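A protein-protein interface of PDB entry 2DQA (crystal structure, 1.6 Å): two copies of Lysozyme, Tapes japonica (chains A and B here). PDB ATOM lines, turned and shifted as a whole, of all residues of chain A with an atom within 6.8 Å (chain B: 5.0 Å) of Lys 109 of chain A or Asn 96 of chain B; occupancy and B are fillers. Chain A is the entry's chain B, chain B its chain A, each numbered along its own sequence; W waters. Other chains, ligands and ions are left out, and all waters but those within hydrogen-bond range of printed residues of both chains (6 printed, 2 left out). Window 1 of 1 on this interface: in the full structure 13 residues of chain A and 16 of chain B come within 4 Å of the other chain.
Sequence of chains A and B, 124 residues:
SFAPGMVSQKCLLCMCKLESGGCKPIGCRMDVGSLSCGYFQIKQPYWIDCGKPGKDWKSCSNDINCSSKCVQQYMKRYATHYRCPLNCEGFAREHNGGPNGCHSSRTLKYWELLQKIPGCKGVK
Of the 13 printed residues of chain A, 6 touch a printed residue of chain B. Of the 15 printed residues of chain B, 6 touch a printed residue of chain A. Hydrophobic or aromatic side chains of chain B that line the printed part of chain A: Leu 113. Among the printed residues, Asp or Glu carboxylates within 4 Å of a Lys or Arg side-chain nitrogen of the other chain: Lys 109 of chain A with Glu 19 of chain B.
Lys 109 of chain A touches just these residues of chain B: Glu 19 (2.6 Å), Asn 96 (3.9 Å) and Leu 113 (3.9 Å). Asn 96 of chain B touches one residue of chain A. Printed residues of chain B within 4 Å of Leu 113 of chain A: Leu 18 (3.4 Å) and Leu 113 (3.9 Å). Of the printed residues of chain A, Arg 106 of chain B touches Arg 106. Of the printed residues of chain B, Lys 116 of chain A touches Glu 19 (3.9 Å). Of the printed residues of chain A, Leu 18 of chain B touches Leu 113. Leu 18 of chain A touches none of the printed residues of chain B. His 95 of chain B touches none of the printed residues of chain A. The nearest printed residue of chain A that does not touch Asn 96 of chain B is Arg 106 of chain A (6.5 Å).
Among the printed residues, merely in contact across the chains: Arg 106 of chain A with Arg 106 of chain B, Lys 109 of chain A with Asn 96 of chain B, Lys 109 of chain A with Leu 113 of chain B, Tyr 110 of chain A with Leu 113 of chain B, Glu 112 of chain A with Asp 31 of chain B, Leu 113 of chain A with Leu 18 of chain B, Leu 113 of chain A with Leu 113 of chain B and Lys 116 of chain A with Glu 19 of chain B.
The side-chain amino group of Lys 109 of chain A lies within salt-bridge range of the side-chain carboxylate of Glu 19 of chain B (2.6 Å).
Arg 106 of chain B touches its own counterpart, Arg 106 of chain A. Tyr 110 of chain A touches Leu 113 of chain B, but with the chains exchanged Leu 113 of chain A does not touch Tyr 110 of chain B (8.1 Å). Leu 113 of chain A touches Leu 18 of chain B, but with the chains exchanged Leu 18 of chain A does not touch Leu 113 of chain B (4.7 Å). Leu 113 of chain A touches its own counterpart, Leu 113 of chain B. 6 positions are printed for both chains. Of the 9 pairs that touch across the chains among the printed residues, 2 have their exchanged pair printed and touching as well.
OE2 of Glu 19 of chain B lies within hydrogen-bond range of OH of Tyr 110 of chain B. The side-chain carboxylate (OE1) of Glu 112 of chain A lies within salt-bridge range of the side-chain amino group (NZ) of Lys 109 of chain A, at 3.9 Å. O of Glu 112 of chain A lies within hydrogen-bond range of NZ of Lys 116 of chain A, at 2.8 Å.
Water W3 lies within hydrogen-bond range of O of Leu 18 of chain B, NZ of Lys 116 of chain A and O of Glu 19 of chain B. Water W6 lies within hydrogen-bond range of the side-chain carboxylate of Glu 19 of chain B, the side-chain amide oxygen of Asn 96 of chain B and the side-chain amino group of Lys 109 of chain A. Water W4 lies within hydrogen-bond range of the backbone carbonyl oxygen of Gln 41 of chain B and the side-chain amino group of Lys 109 of chain A. Water W5 bridges O of Lys 109 of chain A (2.8 Å) and O of Leu 18 of chain B (3.4 Å). Water W2 lies within hydrogen-bond range of O of Glu 19 of chain B and OE1 of Glu 112 of chain A. Water W1 lies within hydrogen-bond range of the side-chain amide oxygen (OE1) of Gln 41 of chain B (3.1 Å), the side-chain amino group (NZ) of Lys 116 of chain A (3.1 Å) and the side-chain carboxylate (OE1) of Glu 112 of chain A (3.1 Å).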
ATOM      1  N   LEU A  18       7.732  20.761   9.605  1.00  0.00           N
ATOM      2  CA  LEU A  18       6.847  20.107  10.560  1.00  0.00           C
ATOM      3  C   LEU A  18       5.658  20.984  10.957  1.00  0.00           C
ATOM      4  O   LEU A  18       4.518  20.515  10.997  1.00  0.00           O
ATOM      5  CB  LEU A  18       7.619  19.692  11.817  1.00  0.00           C
ATOM      6  CG  LEU A  18       6.903  18.804  12.835  1.00  0.00           C
ATOM      7  CD1 LEU A  18       6.215  17.623  12.165  1.00  0.00           C
ATOM      8  CD2 LEU A  18       7.886  18.322  13.884  1.00  0.00           C
ATOM      9  N   ASN A  96       8.443  23.594  21.001  1.00  0.00           N
ATOM     10  CA  ASN A  96       7.242  22.799  21.258  1.00  0.00           C
ATOM     11  C   ASN A  96       6.683  22.968  22.672  1.00  0.00           C
ATOM     12  O   ASN A  96       5.464  22.955  22.866  1.00  0.00           O
ATOM     13  CB  ASN A  96       7.525  21.320  20.971  1.00  0.00           C
ATOM     14  CG  ASN A  96       6.307  20.440  21.162  1.00  0.00           C
ATOM     15  OD1 ASN A  96       6.291  19.575  22.038  1.00  0.00           O
ATOM     16  ND2 ASN A  96       5.287  20.646  20.333  1.00  0.00           N
ATOM     17  N   SER A 105       9.646  15.852  29.258  1.00  0.00           N
ATOM     18  CA  SER A 105       9.561  14.611  28.483  1.00  0.00           C
ATOM     19  C   SER A 105       8.488  14.643  27.388  1.00  0.00           C
ATOM     20  O   SER A 105       8.577  13.897  26.410  1.00  0.00           O
ATOM     21  CB  SER A 105       9.329  13.414  29.413  1.00  0.00           C
ATOM     22  OG  SER A 105       8.118  13.558  30.133  1.00  0.00           O
ATOM     23  N   ARG A 106       7.500  15.517  27.559  1.00  0.00           N
ATOM     24  CA  ARG A 106       6.356  15.634  26.652  1.00  0.00           C
ATOM     25  C   ARG A 106       6.761  16.118  25.258  1.00  0.00           C
ATOM     26  O   ARG A 106       6.098  15.809  24.266  1.00  0.00           O
ATOM     27  CB  ARG A 106       5.304  16.581  27.246  1.00  0.00           C
ATOM     28  CG  ARG A 106       4.704  16.143  28.594  1.00  0.00           C
ATOM     29  CD  ARG A 106       5.730  16.163  29.726  1.00  0.00           C
ATOM     30  NE  ARG A 106       5.142  16.407  31.040  1.00  0.00           N
ATOM     31  CZ  ARG A 106       5.849  16.609  32.150  1.00  0.00           C
ATOM     32  NH1 ARG A 106       7.177  16.599  32.116  1.00  0.00           N
ATOM     33  NH2 ARG A 106       5.227  16.825  33.301  1.00  0.00           N
ATOM     34  N   THR A 107       7.861  16.865  25.196  1.00  0.00           N
ATOM     35  CA  THR A 107       8.335  17.467  23.944  1.00  0.00           C
ATOM     36  C   THR A 107       9.153  16.491  23.097  1.00  0.00           C
ATOM     37  O   THR A 107       9.561  16.818  21.980  1.00  0.00           O
ATOM     38  CB  THR A 107       9.191  18.725  24.208  1.00  0.00           C
ATOM     39  OG1 THR A 107      10.316  18.376  25.025  1.00  0.00           O
ATOM     40  CG2 THR A 107       8.372  19.793  24.911  1.00  0.00           C
ATOM     41  N   LEU A 108       9.395  15.294  23.625  1.00  0.00           N
ATOM     42  CA  LEU A 108      10.203  14.304  22.915  1.00  0.00           C
ATOM     43  C   LEU A 108       9.536  13.782  21.643  1.00  0.00           C
ATOM     44  O   LEU A 108      10.213  13.582  20.635  1.00  0.00           O
ATOM     45  CB  LEU A 108      10.615  13.154  23.842  1.00  0.00           C
ATOM     46  CG  LEU A 108      11.721  13.475  24.853  1.00  0.00           C
ATOM     47  CD1 LEU A 108      11.830  12.378  25.907  1.00  0.00           C
ATOM     48  CD2 LEU A 108      13.067  13.700  24.165  1.00  0.00           C
ATOM     49  N   LYS A 109       8.218  13.577  21.683  1.00  0.00           N
ATOM     50  CA  LYS A 109       7.476  13.126  20.498  1.00  0.00           C
ATOM     51  C   LYS A 109       7.693  14.064  19.313  1.00  0.00           C
ATOM     52  O   LYS A 109       7.884  13.613  18.184  1.00  0.00           O
ATOM     53  CB  LYS A 109       5.975  12.979  20.783  1.00  0.00           C
ATOM     54  CG  LYS A 109       5.578  11.715  21.544  1.00  0.00           C
ATOM     55  CD  LYS A 109       5.646  10.470  20.668  1.00  0.00           C
ATOM     56  CE  LYS A 109       5.320   9.234  21.482  1.00  0.00           C
ATOM     57  NZ  LYS A 109       5.570   7.977  20.734  1.00  0.00           N
ATOM     58  N   TYR A 110       7.666  15.368  19.592  1.00  0.00           N
ATOM     59  CA  TYR A 110       7.929  16.398  18.588  1.00  0.00           C
ATOM     60  C   TYR A 110       9.326  16.224  17.981  1.00  0.00           C
ATOM     61  O   TYR A 110       9.484  16.228  16.759  1.00  0.00           O
ATOM     62  CB  TYR A 110       7.775  17.782  19.228  1.00  0.00           C
ATOM     63  CG  TYR A 110       7.990  18.953  18.294  1.00  0.00           C
ATOM     64  CD1 TYR A 110       6.933  19.494  17.569  1.00  0.00           C
ATOM     65  CD2 TYR A 110       9.250  19.537  18.162  1.00  0.00           C
ATOM     66  CE1 TYR A 110       7.134  20.579  16.716  1.00  0.00           C
ATOM     67  CE2 TYR A 110       9.460  20.615  17.314  1.00  0.00           C
ATOM     68  CZ  TYR A 110       8.398  21.134  16.598  1.00  0.00           C
ATOM     69  OH  TYR A 110       8.613  22.206  15.762  1.00  0.00           O
ATOM     70  N   TRP A 111      10.328  16.060  18.842  1.00  0.00           N
ATOM     71  CA  TRP A 111      11.712  15.855  18.404  1.00  0.00           C
ATOM     72  C   TRP A 111      11.849  14.567  17.592  1.00  0.00           C
ATOM     73  O   TRP A 111      12.505  14.554  16.550  1.00  0.00           O
ATOM     74  CB  TRP A 111      12.663  15.858  19.608  1.00  0.00           C
ATOM     75  CG  TRP A 111      14.083  15.425  19.317  1.00  0.00           C
ATOM     76  CD1 TRP A 111      14.763  14.409  19.924  1.00  0.00           C
ATOM     77  CD2 TRP A 111      14.990  16.000  18.362  1.00  0.00           C
ATOM     78  NE1 TRP A 111      16.036  14.313  19.409  1.00  0.00           N
ATOM     79  CE2 TRP A 111      16.199  15.271  18.444  1.00  0.00           C
ATOM     80  CE3 TRP A 111      14.896  17.052  17.439  1.00  0.00           C
ATOM     81  CZ2 TRP A 111      17.310  15.564  17.643  1.00  0.00           C
ATOM     82  CZ3 TRP A 111      16.000  17.341  16.639  1.00  0.00           C
ATOM     83  CH2 TRP A 111      17.192  16.597  16.749  1.00  0.00           C
ATOM     84  N   GLU A 112      11.201  13.502  18.058  1.00  0.00           N
ATOM     85  CA  GLU A 112      11.174  12.224  17.340  1.00  0.00           C
ATOM     86  C   GLU A 112      10.574  12.369  15.934  1.00  0.00           C
ATOM     87  O   GLU A 112      11.115  11.823  14.969  1.00  0.00           O
ATOM     88  CB  GLU A 112      10.415  11.160  18.145  1.00  0.00           C
ATOM     89  CG  GLU A 112      11.094  10.732  19.452  1.00  0.00           C
ATOM     90  CD  GLU A 112      10.147  10.003  20.405  1.00  0.00           C
ATOM     91  OE1 GLU A 112       9.119   9.454  19.944  1.00  0.00           O
ATOM     92  OE2 GLU A 112      10.431   9.976  21.624  1.00  0.00           O
ATOM     93  N   LEU A 113       9.474  13.116  15.820  1.00  0.00           N
ATOM     94  CA  LEU A 113       8.828  13.336  14.524  1.00  0.00           C
ATOM     95  C   LEU A 113       9.656  14.218  13.595  1.00  0.00           C
ATOM     96  O   LEU A 113       9.761  13.942  12.405  1.00  0.00           O
ATOM     97  CB  LEU A 113       7.414  13.905  14.695  1.00  0.00           C
ATOM     98  CG  LEU A 113       6.549  14.057  13.432  1.00  0.00           C
ATOM     99  CD1 LEU A 113       6.395  12.736  12.678  1.00  0.00           C
ATOM    100  CD2 LEU A 113       5.180  14.625  13.783  1.00  0.00           C
ATOM    101  N   LEU A 114      10.252  15.273  14.150  1.00  0.00           N
ATOM    102  CA  LEU A 114      11.094  16.182  13.376  1.00  0.00           C
ATOM    103  C   LEU A 114      12.190  15.421  12.629  1.00  0.00           C
ATOM    104  O   LEU A 114      12.426  15.668  11.445  1.00  0.00           O
ATOM    105  CB  LEU A 114      11.710  17.249  14.291  1.00  0.00           C
ATOM    106  CG  LEU A 114      12.496  18.393  13.645  1.00  0.00           C
ATOM    107  CD1 LEU A 114      12.410  19.632  14.515  1.00  0.00           C
ATOM    108  CD2 LEU A 114      13.952  18.005  13.406  1.00  0.00           C
ATOM    109  N   LYS A 116      12.270  12.487  11.529  1.00  0.00           N
ATOM    110  CA  LYS A 116      11.766  11.569  10.504  1.00  0.00           C
ATOM    111  C   LYS A 116      11.377  12.274   9.201  1.00  0.00           C
ATOM    112  O   LYS A 116      11.070  11.621   8.200  1.00  0.00           O
ATOM    113  CB  LYS A 116      10.601  10.734  11.051  1.00  0.00           C
ATOM    114  CG  LYS A 116      10.986   9.819  12.211  1.00  0.00           C
ATOM    115  CD  LYS A 116       9.807   8.980  12.688  1.00  0.00           C
ATOM    116  CE  LYS A 116      10.131   8.230  13.968  1.00  0.00           C
ATOM    117  NZ  LYS A 116      10.259   9.160  15.120  1.00  0.00           N
ATOM    118  N   LEU B  18       2.153   9.997  12.491  1.00  0.00           N
ATOM    119  CA  LEU B  18       2.863  10.678  13.577  1.00  0.00           C
ATOM    120  C   LEU B  18       3.889   9.769  14.248  1.00  0.00           C
ATOM    121  O   LEU B  18       5.058  10.146  14.404  1.00  0.00           O
ATOM    122  CB  LEU B  18       1.880  11.216  14.628  1.00  0.00           C
ATOM    123  CG  LEU B  18       2.445  12.070  15.778  1.00  0.00           C
ATOM    124  CD1 LEU B  18       1.355  12.937  16.373  1.00  0.00           C
ATOM    125  CD2 LEU B  18       3.116  11.242  16.881  1.00  0.00           C
ATOM    126  N   GLU B  19       3.458   8.580  14.650  1.00  0.00           N
ATOM    127  CA  GLU B  19       4.314   7.704  15.446  1.00  0.00           C
ATOM    128  C   GLU B  19       5.559   7.207  14.719  1.00  0.00           C
ATOM    129  O   GLU B  19       6.642   7.173  15.306  1.00  0.00           O
ATOM    130  CB  GLU B  19       3.511   6.533  16.021  1.00  0.00           C
ATOM    131  CG  GLU B  19       2.463   6.944  17.062  1.00  0.00           C
ATOM    132  CD  GLU B  19       3.056   7.433  18.383  1.00  0.00           C
ATOM    133  OE1 GLU B  19       4.294   7.436  18.547  1.00  0.00           O
ATOM    134  OE2 GLU B  19       2.265   7.808  19.274  1.00  0.00           O
ATOM    135  N   ASP B  31      12.540   5.622  24.231  1.00  0.00           N
ATOM    136  CA  ASP B  31      11.889   6.870  24.628  1.00  0.00           C
ATOM    137  C   ASP B  31      11.246   6.711  26.006  1.00  0.00           C
ATOM    138  O   ASP B  31      10.417   5.815  26.218  1.00  0.00           O
ATOM    139  CB  ASP B  31      10.859   7.322  23.583  1.00  0.00           C
ATOM    140  CG  ASP B  31       9.822   6.256  23.273  1.00  0.00           C
ATOM    141  OD1 ASP B  31      10.146   5.049  23.347  1.00  0.00           O
ATOM    142  OD2 ASP B  31       8.674   6.629  22.954  1.00  0.00           O
ATOM    143  N   GLN B  41       4.342   2.831  17.387  1.00  0.00           N
ATOM    144  CA  GLN B  41       5.263   2.981  18.519  1.00  0.00           C
ATOM    145  C   GLN B  41       4.676   2.424  19.823  1.00  0.00           C
ATOM    146  O   GLN B  41       4.524   3.122  20.834  1.00  0.00           O
ATOM    147  CB  GLN B  41       5.742   4.432  18.638  1.00  0.00           C
ATOM    148  CG  GLN B  41       6.665   4.826  17.491  1.00  0.00           C
ATOM    149  CD  GLN B  41       8.024   4.152  17.581  1.00  0.00           C
ATOM    150  OE1 GLN B  41       8.864   4.537  18.398  1.00  0.00           O
ATOM    151  NE2 GLN B  41       8.242   3.131  16.753  1.00  0.00           N
ATOM    152  N   ALA B  92      -6.346   9.135  20.586  1.00  0.00           N
ATOM    153  CA  ALA B  92      -4.959   9.612  20.504  1.00  0.00           C
ATOM    154  C   ALA B  92      -4.369   9.855  21.895  1.00  0.00           C
ATOM    155  O   ALA B  92      -3.218   9.490  22.174  1.00  0.00           O
ATOM    156  CB  ALA B  92      -4.886  10.885  19.668  1.00  0.00           C
ATOM    157  N   ARG B  93      -5.167  10.463  22.771  1.00  0.00           N
ATOM    158  CA  ARG B  93      -4.716  10.774  24.128  1.00  0.00           C
ATOM    159  C   ARG B  93      -4.536   9.509  24.977  1.00  0.00           C
ATOM    160  O   ARG B  93      -3.627   9.433  25.804  1.00  0.00           O
ATOM    161  CB  ARG B  93      -5.651  11.796  24.786  1.00  0.00           C
ATOM    162  CG  ARG B  93      -5.573  13.167  24.108  1.00  0.00           C
ATOM    163  CD  ARG B  93      -6.580  14.137  24.680  1.00  0.00           C
ATOM    164  NE  ARG B  93      -6.219  14.527  26.041  1.00  0.00           N
ATOM    165  CZ  ARG B  93      -6.988  15.254  26.847  1.00  0.00           C
ATOM    166  NH1 ARG B  93      -8.184  15.666  26.441  1.00  0.00           N
ATOM    167  NH2 ARG B  93      -6.562  15.558  28.067  1.00  0.00           N
ATOM    168  N   GLU B  94      -5.393   8.515  24.749  1.00  0.00           N
ATOM    169  CA  GLU B  94      -5.221   7.192  25.358  1.00  0.00           C
ATOM    170  C   GLU B  94      -3.935   6.534  24.873  1.00  0.00           C
ATOM    171  O   GLU B  94      -3.160   5.989  25.663  1.00  0.00           O
ATOM    172  CB  GLU B  94      -6.398   6.285  25.010  1.00  0.00           C
ATOM    173  CG  GLU B  94      -7.694   6.670  25.686  1.00  0.00           C
ATOM    174  CD  GLU B  94      -7.683   6.339  27.155  1.00  0.00           C
ATOM    175  OE1 GLU B  94      -8.029   5.192  27.509  1.00  0.00           O
ATOM    176  OE2 GLU B  94      -7.332   7.234  27.949  1.00  0.00           O
ATOM    177  N   HIS B  95      -3.718   6.581  23.564  1.00  0.00           N
ATOM    178  CA  HIS B  95      -2.536   5.973  22.976  1.00  0.00           C
ATOM    179  C   HIS B  95      -1.263   6.547  23.582  1.00  0.00           C
ATOM    180  O   HIS B  95      -0.363   5.802  23.971  1.00  0.00           O
ATOM    181  CB  HIS B  95      -2.536   6.167  21.468  1.00  0.00           C
ATOM    182  CG  HIS B  95      -1.600   5.249  20.753  1.00  0.00           C
ATOM    183  ND1 HIS B  95      -0.426   5.682  20.175  1.00  0.00           N
ATOM    184  CD2 HIS B  95      -1.663   3.916  20.527  1.00  0.00           C
ATOM    185  CE1 HIS B  95       0.189   4.656  19.616  1.00  0.00           C
ATOM    186  NE2 HIS B  95      -0.538   3.572  19.817  1.00  0.00           N
ATOM    187  N   ASN B  96      -1.205   7.874  23.682  1.00  0.00           N
ATOM    188  CA  ASN B  96      -0.026   8.545  24.214  1.00  0.00           C
ATOM    189  C   ASN B  96       0.091   8.485  25.742  1.00  0.00           C
ATOM    190  O   ASN B  96       1.201   8.407  26.280  1.00  0.00           O
ATOM    191  CB  ASN B  96      -0.004  10.002  23.752  1.00  0.00           C
ATOM    192  CG  ASN B  96       1.251  10.730  24.180  1.00  0.00           C
ATOM    193  OD1 ASN B  96       2.362  10.399  23.740  1.00  0.00           O
ATOM    194  ND2 ASN B  96       1.086  11.728  25.031  1.00  0.00           N
ATOM    195  N   GLY B  97      -1.047   8.533  26.434  1.00  0.00           N
ATOM    196  CA  GLY B  97      -1.052   8.677  27.891  1.00  0.00           C
ATOM    197  C   GLY B  97      -1.387   7.451  28.717  1.00  0.00           C
ATOM    198  O   GLY B  97      -1.269   7.480  29.945  1.00  0.00           O
ATOM    199  N   GLY B  98      -1.796   6.370  28.060  1.00  0.00           N
ATOM    200  CA  GLY B  98      -2.168   5.149  28.773  1.00  0.00           C
ATOM    201  C   GLY B  98      -3.655   5.059  29.057  1.00  0.00           C
ATOM    202  O   GLY B  98      -4.438   5.819  28.488  1.00  0.00           O
ATOM    203  N   ARG B 106      -1.626  16.576  30.107  1.00  0.00           N
ATOM    204  CA  ARG B 106      -0.330  16.391  29.464  1.00  0.00           C
ATOM    205  C   ARG B 106      -0.455  15.870  28.024  1.00  0.00           C
ATOM    206  O   ARG B 106       0.310  16.263  27.140  1.00  0.00           O
ATOM    207  CB  ARG B 106       0.510  15.445  30.327  1.00  0.00           C
ATOM    208  CG  ARG B 106       1.751  14.868  29.680  1.00  0.00           C
ATOM    209  CD  ARG B 106       2.285  13.691  30.492  1.00  0.00           C
ATOM    210  NE  ARG B 106       1.221  12.749  30.843  1.00  0.00           N
ATOM    211  CZ  ARG B 106       0.784  11.767  30.058  1.00  0.00           C
ATOM    212  NH1 ARG B 106       1.318  11.567  28.857  1.00  0.00           N
ATOM    213  NH2 ARG B 106      -0.191  10.975  30.481  1.00  0.00           N
ATOM    214  N   THR B 107      -1.433  14.996  27.792  1.00  0.00           N
ATOM    215  CA  THR B 107      -1.616  14.387  26.470  1.00  0.00           C
ATOM    216  C   THR B 107      -2.167  15.340  25.406  1.00  0.00           C
ATOM    217  O   THR B 107      -2.213  14.990  24.227  1.00  0.00           O
ATOM    218  CB  THR B 107      -2.529  13.145  26.530  1.00  0.00           C
ATOM    219  OG1 THR B 107      -3.799  13.512  27.081  1.00  0.00           O
ATOM    220  CG2 THR B 107      -1.903  12.055  27.379  1.00  0.00           C
ATOM    221  N   TYR B 110       0.200  15.968  22.556  1.00  0.00           N
ATOM    222  CA  TYR B 110       0.188  14.916  21.550  1.00  0.00           C
ATOM    223  C   TYR B 110      -0.917  15.162  20.529  1.00  0.00           C
ATOM    224  O   TYR B 110      -0.699  15.014  19.333  1.00  0.00           O
ATOM    225  CB  TYR B 110      -0.017  13.559  22.221  1.00  0.00           C
ATOM    226  CG  TYR B 110       0.017  12.382  21.278  1.00  0.00           C
ATOM    227  CD1 TYR B 110      -1.164  11.812  20.806  1.00  0.00           C
ATOM    228  CD2 TYR B 110       1.229  11.823  20.872  1.00  0.00           C
ATOM    229  CE1 TYR B 110      -1.144  10.722  19.952  1.00  0.00           C
ATOM    230  CE2 TYR B 110       1.260  10.727  20.016  1.00  0.00           C
ATOM    231  CZ  TYR B 110       0.069  10.181  19.563  1.00  0.00           C
ATOM    232  OH  TYR B 110       0.075   9.102  18.711  1.00  0.00           O
ATOM    233  N   LEU B 113       0.076  17.941  18.268  1.00  0.00           N
ATOM    234  CA  LEU B 113       1.067  17.494  17.294  1.00  0.00           C
ATOM    235  C   LEU B 113       0.432  16.658  16.189  1.00  0.00           C
ATOM    236  O   LEU B 113       0.769  16.816  15.016  1.00  0.00           O
ATOM    237  CB  LEU B 113       2.171  16.699  17.996  1.00  0.00           C
ATOM    238  CG  LEU B 113       3.350  16.152  17.186  1.00  0.00           C
ATOM    239  CD1 LEU B 113       4.126  17.257  16.479  1.00  0.00           C
ATOM    240  CD2 LEU B 113       4.265  15.371  18.115  1.00  0.00           C
HETATM  241  O   HOH W   1       9.891   7.400  17.685  1.00  0.00           O
HETATM  242  O   HOH W   2       7.440   8.540  17.620  1.00  0.00           O
HETATM  243  O   HOH W   3       7.617  10.187  15.015  1.00  0.00           O
HETATM  244  O   HOH W   4       4.142   5.394  22.272  1.00  0.00           O
HETATM  245  O   HOH W   5       6.833  11.238  17.144  1.00  0.00           O
HETATM  246  O   HOH W   6       2.493   7.722  21.938  1.00  0.00           O
